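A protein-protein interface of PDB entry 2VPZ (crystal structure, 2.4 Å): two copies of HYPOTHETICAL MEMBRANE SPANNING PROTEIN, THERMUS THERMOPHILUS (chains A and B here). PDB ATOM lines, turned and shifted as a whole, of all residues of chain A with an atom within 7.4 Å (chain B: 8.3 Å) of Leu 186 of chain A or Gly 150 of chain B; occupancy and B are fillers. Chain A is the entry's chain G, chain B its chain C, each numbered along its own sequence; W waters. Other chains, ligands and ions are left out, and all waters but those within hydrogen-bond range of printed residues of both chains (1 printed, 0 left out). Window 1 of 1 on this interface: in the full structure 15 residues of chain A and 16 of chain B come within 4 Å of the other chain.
CG of Leu 147 of chain A touches O of Gly 146 of chain B, at 3.4 Å.
Leu 147 of chain B touches Leu 147 of chain A (N to N, 3.7 Å).
CD1 of Leu 186 of chain B touches CA of Gly 150 of chain A, at 3.5 Å.
Ser 129 of chain B touches Leu 185 of chain A (OG to CD1, 3.5 Å).
O of Ala 149 of chain B touches CD2 of Leu 186 of chain A, 3.6 Å away.
Gly 150 of chain B touches Leu 186 of chain A.
Leu 189 of chain A touches Ser 129 of chain B (CD1 to OG, 3.7 Å).
Ala 149 of chain B touches Leu 189 of chain A (O to CD1, 3.8 Å).
Ala 149 of chain B touches Thr 193 of chain A.
Water W1 lies within hydrogen-bond range of O of Ala 136 of chain B (2.7 Å), O of Thr 193 of chain A (3.0 Å) and N of Gly 146 of chain B (3.5 Å).
Leu 186 of chain A touches just these residues of chain B: Ala 149 and Gly 150.
Gly 150 of chain B touches just one residue of chain A: Leu 186.
No residue of chain B comes within 4 Å of Ala 187 of chain A.
Of the printed residues of chain B, Leu 189 of chain A touches Ser 129 and Ala 149.
Of the printed residues of chain B, Thr 193 of chain A touches Ala 149.
Printed residues of chain B within 4 Å of Leu 185 of chain A: Ser 129.
Tyr 210 of chain A touches none of the printed residues of chain B.
Pro 153 of chain B touches none of the printed residues of chain A.
The nearest residue of chain A that does not touch Gly 150 of chain B is Leu 147 of chain A (4.04 Å).
The nearest printed residue of chain A that does not touch Ser 129 of chain B is Leu 188 of chain A (6.5 Å).
Of the 22 printed residues of chain B, 6 touch a printed residue of chain A.
Of the 19 printed residues of chain A, 6 touch a printed residue of chain B.
Printed residues of chain A that touch a printed residue of chain B: Leu 147, Gly 150, Leu 185, Leu 186, Leu 189 and Thr 193.
Hydrophobic or aromatic side chains of chain A that line the printed part of chain B: Leu 147, Leu 185, Leu 186 and Leu 189.
Among the printed residues, no Asp or Glu carboxylate lies within 4 Å of a Lys or Arg side-chain nitrogen of the other chain.
Leu 147 of chain A touches its own counterpart, Leu 147 of chain B.
Gly 150 of chain A touches Leu 186 of chain B, and with the chains exchanged Leu 186 of chain A touches Gly 150 of chain B.
ND2 of Asn 145 of chain B sits close to N of Leu 147 of chain B, 3.0 Å away.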
ATOM      1  N   LEU A 147     -16.966  -8.304  16.644  1.00  0.00           N
ATOM      2  CA  LEU A 147     -17.362  -9.719  16.878  1.00  0.00           C
ATOM      3  C   LEU A 147     -16.762 -10.392  18.137  1.00  0.00           C
ATOM      4  O   LEU A 147     -17.314 -11.375  18.621  1.00  0.00           O
ATOM      5  CB  LEU A 147     -17.089 -10.638  15.663  1.00  0.00           C
ATOM      6  CG  LEU A 147     -18.319 -11.191  14.926  1.00  0.00           C
ATOM      7  CD1 LEU A 147     -17.866 -12.286  13.942  1.00  0.00           C
ATOM      8  CD2 LEU A 147     -19.394 -11.749  15.910  1.00  0.00           C
ATOM      9  N   GLY A 150     -18.951 -10.770  20.962  1.00  0.00           N
ATOM     10  CA  GLY A 150     -19.952 -11.799  20.761  1.00  0.00           C
ATOM     11  C   GLY A 150     -19.336 -13.196  20.800  1.00  0.00           C
ATOM     12  O   GLY A 150     -19.893 -14.130  21.403  1.00  0.00           O
ATOM     13  N   LEU A 151     -18.177 -13.353  20.165  1.00  0.00           N
ATOM     14  CA  LEU A 151     -17.466 -14.629  20.167  1.00  0.00           C
ATOM     15  C   LEU A 151     -16.969 -15.084  21.562  1.00  0.00           C
ATOM     16  O   LEU A 151     -16.879 -16.286  21.809  1.00  0.00           O
ATOM     17  CB  LEU A 151     -16.301 -14.621  19.159  1.00  0.00           C
ATOM     18  CG  LEU A 151     -16.759 -15.118  17.794  1.00  0.00           C
ATOM     19  CD1 LEU A 151     -15.683 -14.959  16.710  1.00  0.00           C
ATOM     20  CD2 LEU A 151     -17.177 -16.584  17.947  1.00  0.00           C
ATOM     21  N   LEU A 154     -20.208 -16.346  23.922  1.00  0.00           N
ATOM     22  CA  LEU A 154     -20.789 -17.580  23.357  1.00  0.00           C
ATOM     23  C   LEU A 154     -19.908 -18.800  23.667  1.00  0.00           C
ATOM     24  O   LEU A 154     -20.372 -19.886  24.053  1.00  0.00           O
ATOM     25  CB  LEU A 154     -21.032 -17.485  21.826  1.00  0.00           C
ATOM     26  CG  LEU A 154     -22.294 -16.775  21.312  1.00  0.00           C
ATOM     27  CD1 LEU A 154     -22.508 -17.107  19.835  1.00  0.00           C
ATOM     28  CD2 LEU A 154     -23.536 -17.204  22.112  1.00  0.00           C
ATOM     29  N   ALA A 180     -23.107 -24.161  20.868  1.00  0.00           N
ATOM     30  CA  ALA A 180     -21.949 -24.601  20.097  1.00  0.00           C
ATOM     31  C   ALA A 180     -22.224 -24.349  18.593  1.00  0.00           C
ATOM     32  O   ALA A 180     -21.285 -24.061  17.857  1.00  0.00           O
ATOM     33  CB  ALA A 180     -21.627 -26.088  20.352  1.00  0.00           C
ATOM     34  N   GLY A 181     -23.479 -24.464  18.148  1.00  0.00           N
ATOM     35  CA  GLY A 181     -23.858 -24.167  16.767  1.00  0.00           C
ATOM     36  C   GLY A 181     -23.792 -22.653  16.514  1.00  0.00           C
ATOM     37  O   GLY A 181     -23.237 -22.180  15.509  1.00  0.00           O
ATOM     38  N   ALA A 182     -24.367 -21.875  17.430  1.00  0.00           N
ATOM     39  CA  ALA A 182     -24.278 -20.411  17.369  1.00  0.00           C
ATOM     40  C   ALA A 182     -22.753 -20.036  17.346  1.00  0.00           C
ATOM     41  O   ALA A 182     -22.324 -19.331  16.437  1.00  0.00           O
ATOM     42  CB  ALA A 182     -24.993 -19.759  18.589  1.00  0.00           C
ATOM     43  N   SER A 183     -21.945 -20.527  18.300  1.00  0.00           N
ATOM     44  CA  SER A 183     -20.466 -20.273  18.387  1.00  0.00           C
ATOM     45  C   SER A 183     -19.657 -20.566  17.098  1.00  0.00           C
ATOM     46  O   SER A 183     -18.813 -19.771  16.645  1.00  0.00           O
ATOM     47  CB  SER A 183     -19.785 -21.105  19.511  1.00  0.00           C
ATOM     48  OG  SER A 183     -19.926 -20.573  20.814  1.00  0.00           O
ATOM     49  N   LEU A 184     -19.905 -21.741  16.538  1.00  0.00           N
ATOM     50  CA  LEU A 184     -19.234 -22.204  15.335  1.00  0.00           C
ATOM     51  C   LEU A 184     -19.646 -21.458  14.062  1.00  0.00           C
ATOM     52  O   LEU A 184     -18.839 -21.339  13.138  1.00  0.00           O
ATOM     53  CB  LEU A 184     -19.451 -23.710  15.141  1.00  0.00           C
ATOM     54  CG  LEU A 184     -18.823 -24.761  16.055  1.00  0.00           C
ATOM     55  CD1 LEU A 184     -19.235 -26.150  15.521  1.00  0.00           C
ATOM     56  CD2 LEU A 184     -17.273 -24.622  16.121  1.00  0.00           C
ATOM     57  N   LEU A 185     -20.894 -20.986  13.990  1.00  0.00           N
ATOM     58  CA  LEU A 185     -21.357 -20.260  12.798  1.00  0.00           C
ATOM     59  C   LEU A 185     -20.802 -18.835  12.788  1.00  0.00           C
ATOM     60  O   LEU A 185     -20.433 -18.346  11.722  1.00  0.00           O
ATOM     61  CB  LEU A 185     -22.901 -20.224  12.618  1.00  0.00           C
ATOM     62  CG  LEU A 185     -23.444 -19.430  11.398  1.00  0.00           C
ATOM     63  CD1 LEU A 185     -23.074 -20.083  10.042  1.00  0.00           C
ATOM     64  CD2 LEU A 185     -24.971 -19.302  11.496  1.00  0.00           C
ATOM     65  N   LEU A 186     -20.744 -18.163  13.943  1.00  0.00           N
ATOM     66  CA  LEU A 186     -20.157 -16.816  14.013  1.00  0.00           C
ATOM     67  C   LEU A 186     -18.638 -16.927  13.761  1.00  0.00           C
ATOM     68  O   LEU A 186     -18.039 -16.025  13.168  1.00  0.00           O
ATOM     69  CB  LEU A 186     -20.349 -16.110  15.384  1.00  0.00           C
ATOM     70  CG  LEU A 186     -21.732 -15.927  16.024  1.00  0.00           C
ATOM     71  CD1 LEU A 186     -21.724 -14.775  17.059  1.00  0.00           C
ATOM     72  CD2 LEU A 186     -22.761 -15.668  14.924  1.00  0.00           C
ATOM     73  N   ALA A 187     -18.018 -18.021  14.202  1.00  0.00           N
ATOM     74  CA  ALA A 187     -16.567 -18.213  14.038  1.00  0.00           C
ATOM     75  C   ALA A 187     -16.147 -18.365  12.572  1.00  0.00           C
ATOM     76  O   ALA A 187     -15.037 -17.994  12.177  1.00  0.00           O
ATOM     77  CB  ALA A 187     -16.058 -19.425  14.882  1.00  0.00           C
ATOM     78  N   LEU A 188     -17.070 -18.886  11.777  1.00  0.00           N
ATOM     79  CA  LEU A 188     -16.929 -19.084  10.331  1.00  0.00           C
ATOM     80  C   LEU A 188     -17.091 -17.737   9.551  1.00  0.00           C
ATOM     81  O   LEU A 188     -16.404 -17.482   8.543  1.00  0.00           O
ATOM     82  CB  LEU A 188     -17.985 -20.092   9.852  1.00  0.00           C
ATOM     83  CG  LEU A 188     -18.088 -20.445   8.373  1.00  0.00           C
ATOM     84  CD1 LEU A 188     -16.812 -21.151   7.896  1.00  0.00           C
ATOM     85  CD2 LEU A 188     -19.313 -21.331   8.157  1.00  0.00           C
ATOM     86  N   LEU A 189     -18.015 -16.895  10.025  1.00  0.00           N
ATOM     87  CA  LEU A 189     -18.324 -15.595   9.425  1.00  0.00           C
ATOM     88  C   LEU A 189     -17.260 -14.530   9.774  1.00  0.00           C
ATOM     89  O   LEU A 189     -17.010 -13.609   8.992  1.00  0.00           O
ATOM     90  CB  LEU A 189     -19.754 -15.132   9.822  1.00  0.00           C
ATOM     91  CG  LEU A 189     -20.944 -16.039   9.453  1.00  0.00           C
ATOM     92  CD1 LEU A 189     -22.284 -15.352   9.785  1.00  0.00           C
ATOM     93  CD2 LEU A 189     -20.898 -16.406   7.963  1.00  0.00           C
ATOM     94  N   TYR A 190     -16.628 -14.660  10.933  1.00  0.00           N
ATOM     95  CA  TYR A 190     -15.569 -13.737  11.378  1.00  0.00           C
ATOM     96  C   TYR A 190     -14.538 -13.310  10.247  1.00  0.00           C
ATOM     97  O   TYR A 190     -14.398 -12.103   9.969  1.00  0.00           O
ATOM     98  CB  TYR A 190     -14.845 -14.318  12.611  1.00  0.00           C
ATOM     99  CG  TYR A 190     -13.666 -13.482  13.056  1.00  0.00           C
ATOM    100  CD1 TYR A 190     -13.840 -12.174  13.521  1.00  0.00           C
ATOM    101  CD2 TYR A 190     -12.365 -13.978  12.939  1.00  0.00           C
ATOM    102  CE1 TYR A 190     -12.739 -11.374  13.854  1.00  0.00           C
ATOM    103  CE2 TYR A 190     -11.260 -13.195  13.264  1.00  0.00           C
ATOM    104  CZ  TYR A 190     -11.449 -11.897  13.718  1.00  0.00           C
ATOM    105  OH  TYR A 190     -10.332 -11.160  14.018  1.00  0.00           O
ATOM    106  N   PRO A 191     -13.793 -14.259   9.607  1.00  0.00           N
ATOM    107  CA  PRO A 191     -12.849 -13.859   8.539  1.00  0.00           C
ATOM    108  C   PRO A 191     -13.411 -12.933   7.402  1.00  0.00           C
ATOM    109  O   PRO A 191     -12.685 -12.101   6.816  1.00  0.00           O
ATOM    110  CB  PRO A 191     -12.396 -15.192   7.940  1.00  0.00           C
ATOM    111  CG  PRO A 191     -12.393 -16.129   9.123  1.00  0.00           C
ATOM    112  CD  PRO A 191     -13.591 -15.670   9.979  1.00  0.00           C
ATOM    113  N   THR A 193     -15.576 -10.627   7.589  1.00  0.00           N
ATOM    114  CA  THR A 193     -15.892  -9.411   8.302  1.00  0.00           C
ATOM    115  C   THR A 193     -14.695  -8.427   8.398  1.00  0.00           C
ATOM    116  O   THR A 193     -14.854  -7.249   8.751  1.00  0.00           O
ATOM    117  CB  THR A 193     -16.311  -9.900   9.708  1.00  0.00           C
ATOM    118  OG1 THR A 193     -17.723  -9.892   9.852  1.00  0.00           O
ATOM    119  CG2 THR A 193     -15.573  -9.154  10.788  1.00  0.00           C
ATOM    120  N   TYR A 210      -6.985 -22.437  12.733  1.00  0.00           N
ATOM    121  CA  TYR A 210      -8.340 -21.865  12.726  1.00  0.00           C
ATOM    122  C   TYR A 210      -9.365 -22.866  12.119  1.00  0.00           C
ATOM    123  O   TYR A 210     -10.375 -23.177  12.739  1.00  0.00           O
ATOM    124  CB  TYR A 210      -8.392 -20.561  11.921  1.00  0.00           C
ATOM    125  CG  TYR A 210      -9.568 -19.701  12.264  1.00  0.00           C
ATOM    126  CD1 TYR A 210      -9.459 -18.711  13.228  1.00  0.00           C
ATOM    127  CD2 TYR A 210     -10.829 -19.936  11.685  1.00  0.00           C
ATOM    128  CE1 TYR A 210     -10.568 -17.967  13.628  1.00  0.00           C
ATOM    129  CE2 TYR A 210     -11.960 -19.202  12.074  1.00  0.00           C
ATOM    130  CZ  TYR A 210     -11.825 -18.216  13.048  1.00  0.00           C
ATOM    131  OH  TYR A 210     -12.931 -17.496  13.440  1.00  0.00           O
ATOM    132  N   LEU A 214     -12.485 -25.408  13.848  1.00  0.00           N
ATOM    133  CA  LEU A 214     -13.854 -25.238  13.330  1.00  0.00           C
ATOM    134  C   LEU A 214     -14.363 -26.656  13.025  1.00  0.00           C
ATOM    135  O   LEU A 214     -15.490 -27.007  13.385  1.00  0.00           O
ATOM    136  CB  LEU A 214     -13.950 -24.388  12.032  1.00  0.00           C
ATOM    137  CG  LEU A 214     -13.952 -22.852  11.886  1.00  0.00           C
ATOM    138  CD1 LEU A 214     -14.171 -22.510  10.391  1.00  0.00           C
ATOM    139  CD2 LEU A 214     -15.046 -22.178  12.748  1.00  0.00           C
ATOM    140  N   LEU B 128     -29.644 -17.356   6.783  1.00  0.00           N
ATOM    141  CA  LEU B 128     -29.561 -16.812   8.175  1.00  0.00           C
ATOM    142  C   LEU B 128     -28.315 -15.946   8.351  1.00  0.00           C
ATOM    143  O   LEU B 128     -28.240 -15.086   9.241  1.00  0.00           O
ATOM    144  CB  LEU B 128     -29.480 -17.955   9.216  1.00  0.00           C
ATOM    145  CG  LEU B 128     -30.740 -18.597   9.818  1.00  0.00           C
ATOM    146  CD1 LEU B 128     -30.443 -20.014  10.353  1.00  0.00           C
ATOM    147  CD2 LEU B 128     -31.330 -17.706  10.935  1.00  0.00           C
ATOM    148  N   SER B 129     -27.333 -16.238   7.513  1.00  0.00           N
ATOM    149  CA  SER B 129     -26.023 -15.606   7.498  1.00  0.00           C
ATOM    150  C   SER B 129     -25.825 -14.387   6.583  1.00  0.00           C
ATOM    151  O   SER B 129     -25.022 -13.505   6.893  1.00  0.00           O
ATOM    152  CB  SER B 129     -24.951 -16.661   7.108  1.00  0.00           C
ATOM    153  OG  SER B 129     -24.694 -17.616   8.093  1.00  0.00           O
ATOM    154  N   GLY B 132     -26.629 -10.072   8.000  1.00  0.00           N
ATOM    155  CA  GLY B 132     -25.609  -9.428   8.813  1.00  0.00           C
ATOM    156  C   GLY B 132     -24.361  -9.088   8.006  1.00  0.00           C
ATOM    157  O   GLY B 132     -23.670  -8.088   8.264  1.00  0.00           O
ATOM    158  N   LEU B 133     -24.056  -9.917   7.013  1.00  0.00           N
ATOM    159  CA  LEU B 133     -22.911  -9.665   6.126  1.00  0.00           C
ATOM    160  C   LEU B 133     -23.262  -8.608   5.034  1.00  0.00           C
ATOM    161  O   LEU B 133     -22.361  -7.935   4.533  1.00  0.00           O
ATOM    162  CB  LEU B 133     -22.354 -10.980   5.497  1.00  0.00           C
ATOM    163  CG  LEU B 133     -21.674 -12.036   6.398  1.00  0.00           C
ATOM    164  CD1 LEU B 133     -21.160 -13.221   5.554  1.00  0.00           C
ATOM    165  CD2 LEU B 133     -20.496 -11.412   7.189  1.00  0.00           C
ATOM    166  N   ALA B 136     -22.377  -5.582   7.373  1.00  0.00           N
ATOM    167  CA  ALA B 136     -20.964  -5.694   7.809  1.00  0.00           C
ATOM    168  C   ALA B 136     -19.790  -5.577   6.824  1.00  0.00           C
ATOM    169  O   ALA B 136     -18.672  -5.296   7.231  1.00  0.00           O
ATOM    170  CB  ALA B 136     -20.784  -6.990   8.693  1.00  0.00           C
ATOM    171  N   ASN B 145     -20.501  -2.689  12.121  1.00  0.00           N
ATOM    172  CA  ASN B 145     -19.255  -3.405  12.359  1.00  0.00           C
ATOM    173  C   ASN B 145     -19.458  -4.935  12.431  1.00  0.00           C
ATOM    174  O   ASN B 145     -20.567  -5.444  12.190  1.00  0.00           O
ATOM    175  CB  ASN B 145     -18.541  -2.849  13.622  1.00  0.00           C
ATOM    176  CG  ASN B 145     -19.184  -3.288  14.935  1.00  0.00           C
ATOM    177  OD1 ASN B 145     -18.797  -2.846  16.021  1.00  0.00           O
ATOM    178  ND2 ASN B 145     -20.179  -4.172  14.832  1.00  0.00           N
ATOM    179  N   GLY B 146     -18.366  -5.632  12.729  1.00  0.00           N
ATOM    180  CA  GLY B 146     -18.374  -7.082  12.825  1.00  0.00           C
ATOM    181  C   GLY B 146     -19.495  -7.763  13.602  1.00  0.00           C
ATOM    182  O   GLY B 146     -19.965  -8.807  13.172  1.00  0.00           O
ATOM    183  N   LEU B 147     -19.934  -7.181  14.718  1.00  0.00           N
ATOM    184  CA  LEU B 147     -21.041  -7.737  15.540  1.00  0.00           C
ATOM    185  C   LEU B 147     -22.364  -7.985  14.754  1.00  0.00           C
ATOM    186  O   LEU B 147     -23.218  -8.770  15.184  1.00  0.00           O
ATOM    187  CB  LEU B 147     -21.347  -6.871  16.790  1.00  0.00           C
ATOM    188  CG  LEU B 147     -21.129  -7.311  18.245  1.00  0.00           C
ATOM    189  CD1 LEU B 147     -21.897  -6.363  19.209  1.00  0.00           C
ATOM    190  CD2 LEU B 147     -21.588  -8.770  18.483  1.00  0.00           C
ATOM    191  N   MET B 148     -22.538  -7.271  13.633  1.00  0.00           N
ATOM    192  CA  MET B 148     -23.730  -7.383  12.784  1.00  0.00           C
ATOM    193  C   MET B 148     -23.797  -8.819  12.234  1.00  0.00           C
ATOM    194  O   MET B 148     -24.882  -9.347  11.942  1.00  0.00           O
ATOM    195  CB  MET B 148     -23.705  -6.384  11.612  1.00  0.00           C
ATOM    196  CG  MET B 148     -23.703  -4.897  12.006  1.00  0.00           C
ATOM    197  SD  MET B 148     -25.167  -4.395  12.938  1.00  0.00           S
ATOM    198  CE  MET B 148     -24.439  -4.004  14.559  1.00  0.00           C
ATOM    199  N   ALA B 149     -22.628  -9.432  12.065  1.00  0.00           N
ATOM    200  CA  ALA B 149     -22.542 -10.809  11.608  1.00  0.00           C
ATOM    201  C   ALA B 149     -22.910 -11.772  12.783  1.00  0.00           C
ATOM    202  O   ALA B 149     -23.120 -12.963  12.563  1.00  0.00           O
ATOM    203  CB  ALA B 149     -21.130 -11.133  11.049  1.00  0.00           C
ATOM    204  N   GLY B 150     -22.974 -11.247  14.005  1.00  0.00           N
ATOM    205  CA  GLY B 150     -23.355 -12.036  15.160  1.00  0.00           C
ATOM    206  C   GLY B 150     -24.788 -11.757  15.599  1.00  0.00           C
ATOM    207  O   GLY B 150     -25.569 -12.675  15.937  1.00  0.00           O
ATOM    208  N   LEU B 151     -25.159 -10.481  15.591  1.00  0.00           N
ATOM    209  CA  LEU B 151     -26.494 -10.016  15.946  1.00  0.00           C
ATOM    210  C   LEU B 151     -27.585 -10.468  14.953  1.00  0.00           C
ATOM    211  O   LEU B 151     -28.701 -10.820  15.362  1.00  0.00           O
ATOM    212  CB  LEU B 151     -26.527  -8.478  16.079  1.00  0.00           C
ATOM    213  CG  LEU B 151     -25.888  -7.904  17.354  1.00  0.00           C
ATOM    214  CD1 LEU B 151     -25.941  -6.362  17.356  1.00  0.00           C
ATOM    215  CD2 LEU B 151     -26.608  -8.472  18.595  1.00  0.00           C
ATOM    216  N   PHE B 152     -27.288 -10.504  13.657  1.00  0.00           N
ATOM    217  CA  PHE B 152     -28.340 -10.906  12.759  1.00  0.00           C
ATOM    218  C   PHE B 152     -28.719 -12.421  12.790  1.00  0.00           C
ATOM    219  O   PHE B 152     -29.916 -12.729  12.787  1.00  0.00           O
ATOM    220  CB  PHE B 152     -28.171 -10.227  11.384  1.00  0.00           C
ATOM    221  CG  PHE B 152     -28.698  -8.781  11.332  1.00  0.00           C
ATOM    222  CD1 PHE B 152     -28.075  -7.780  12.074  1.00  0.00           C
ATOM    223  CD2 PHE B 152     -29.863  -8.453  10.605  1.00  0.00           C
ATOM    224  CE1 PHE B 152     -28.579  -6.467  12.115  1.00  0.00           C
ATOM    225  CE2 PHE B 152     -30.391  -7.136  10.632  1.00  0.00           C
ATOM    226  CZ  PHE B 152     -29.747  -6.146  11.389  1.00  0.00           C
ATOM    227  N   PRO B 153     -27.728 -13.358  12.832  1.00  0.00           N
ATOM    228  CA  PRO B 153     -28.069 -14.789  12.912  1.00  0.00           C
ATOM    229  C   PRO B 153     -28.846 -15.178  14.235  1.00  0.00           C
ATOM    230  O   PRO B 153     -29.842 -15.914  14.204  1.00  0.00           O
ATOM    231  CB  PRO B 153     -26.721 -15.495  12.824  1.00  0.00           C
ATOM    232  CG  PRO B 153     -25.931 -14.611  11.893  1.00  0.00           C
ATOM    233  CD  PRO B 153     -26.380 -13.179  12.264  1.00  0.00           C
ATOM    234  N   LEU B 154     -28.384 -14.698  15.388  1.00  0.00           N
ATOM    235  CA  LEU B 154     -29.024 -14.981  16.675  1.00  0.00           C
ATOM    236  C   LEU B 154     -30.439 -14.398  16.785  1.00  0.00           C
ATOM    237  O   LEU B 154     -31.324 -14.970  17.430  1.00  0.00           O
ATOM    238  CB  LEU B 154     -28.175 -14.468  17.868  1.00  0.00           C
ATOM    239  CG  LEU B 154     -26.939 -15.298  18.294  1.00  0.00           C
ATOM    240  CD1 LEU B 154     -25.913 -14.409  19.038  1.00  0.00           C
ATOM    241  CD2 LEU B 154     -27.359 -16.507  19.166  1.00  0.00           C
ATOM    242  N   THR B 155     -30.668 -13.272  16.134  1.00  0.00           N
ATOM    243  CA  THR B 155     -31.963 -12.609  16.194  1.00  0.00           C
ATOM    244  C   THR B 155     -33.025 -13.256  15.283  1.00  0.00           C
ATOM    245  O   THR B 155     -34.235 -13.229  15.593  1.00  0.00           O
ATOM    246  CB  THR B 155     -31.761 -11.068  15.930  1.00  0.00           C
ATOM    247  OG1 THR B 155     -32.104 -10.333  17.103  1.00  0.00           O
ATOM    248  CG2 THR B 155     -32.568 -10.616  14.740  1.00  0.00           C
ATOM    249  N   ALA B 156     -32.573 -13.871  14.193  1.00  0.00           N
ATOM    250  CA  ALA B 156     -33.439 -14.576  13.246  1.00  0.00           C
ATOM    251  C   ALA B 156     -33.959 -15.874  13.925  1.00  0.00           C
ATOM    252  O   ALA B 156     -35.055 -16.363  13.610  1.00  0.00           O
ATOM    253  CB  ALA B 156     -32.639 -14.920  11.937  1.00  0.00           C
ATOM    254  N   LEU B 157     -33.180 -16.385  14.881  1.00  0.00           N
ATOM    255  CA  LEU B 157     -33.532 -17.572  15.666  1.00  0.00           C
ATOM    256  C   LEU B 157     -34.583 -17.210  16.744  1.00  0.00           C
ATOM    257  O   LEU B 157     -35.553 -17.944  16.941  1.00  0.00           O
ATOM    258  CB  LEU B 157     -32.272 -18.238  16.267  1.00  0.00           C
ATOM    259  CG  LEU B 157     -31.279 -18.786  15.208  1.00  0.00           C
ATOM    260  CD1 LEU B 157     -29.948 -19.241  15.855  1.00  0.00           C
ATOM    261  CD2 LEU B 157     -31.954 -19.932  14.417  1.00  0.00           C
ATOM    262  N   ALA B 182     -28.678 -14.722  24.862  1.00  0.00           N
ATOM    263  CA  ALA B 182     -27.469 -14.487  24.062  1.00  0.00           C
ATOM    264  C   ALA B 182     -27.623 -13.163  23.265  1.00  0.00           C
ATOM    265  O   ALA B 182     -26.798 -12.250  23.411  1.00  0.00           O
ATOM    266  CB  ALA B 182     -27.227 -15.684  23.090  1.00  0.00           C
ATOM    267  N   SER B 183     -28.687 -13.061  22.461  1.00  0.00           N
ATOM    268  CA  SER B 183     -29.016 -11.869  21.654  1.00  0.00           C
ATOM    269  C   SER B 183     -29.069 -10.586  22.508  1.00  0.00           C
ATOM    270  O   SER B 183     -28.525  -9.551  22.114  1.00  0.00           O
ATOM    271  CB  SER B 183     -30.363 -12.011  20.905  1.00  0.00           C
ATOM    272  OG  SER B 183     -30.472 -13.200  20.149  1.00  0.00           O
ATOM    273  N   LEU B 186     -25.334  -9.622  23.781  1.00  0.00           N
ATOM    274  CA  LEU B 186     -24.542  -9.027  22.679  1.00  0.00           C
ATOM    275  C   LEU B 186     -25.106  -7.619  22.246  1.00  0.00           C
ATOM    276  O   LEU B 186     -24.336  -6.711  21.907  1.00  0.00           O
ATOM    277  CB  LEU B 186     -24.419  -9.998  21.457  1.00  0.00           C
ATOM    278  CG  LEU B 186     -24.023 -11.484  21.641  1.00  0.00           C
ATOM    279  CD1 LEU B 186     -23.413 -12.081  20.340  1.00  0.00           C
ATOM    280  CD2 LEU B 186     -23.033 -11.654  22.814  1.00  0.00           C
ATOM    281  N   ALA B 187     -26.431  -7.441  22.292  1.00  0.00           N
ATOM    282  CA  ALA B 187     -27.083  -6.176  21.928  1.00  0.00           C
ATOM    283  C   ALA B 187     -26.777  -5.043  22.939  1.00  0.00           C
ATOM    284  O   ALA B 187     -26.698  -3.859  22.574  1.00  0.00           O
ATOM    285  CB  ALA B 187     -28.632  -6.352  21.781  1.00  0.00           C
HETATM  286  O   HOH W   1     -17.223  -5.530   9.458  1.00  0.00           O
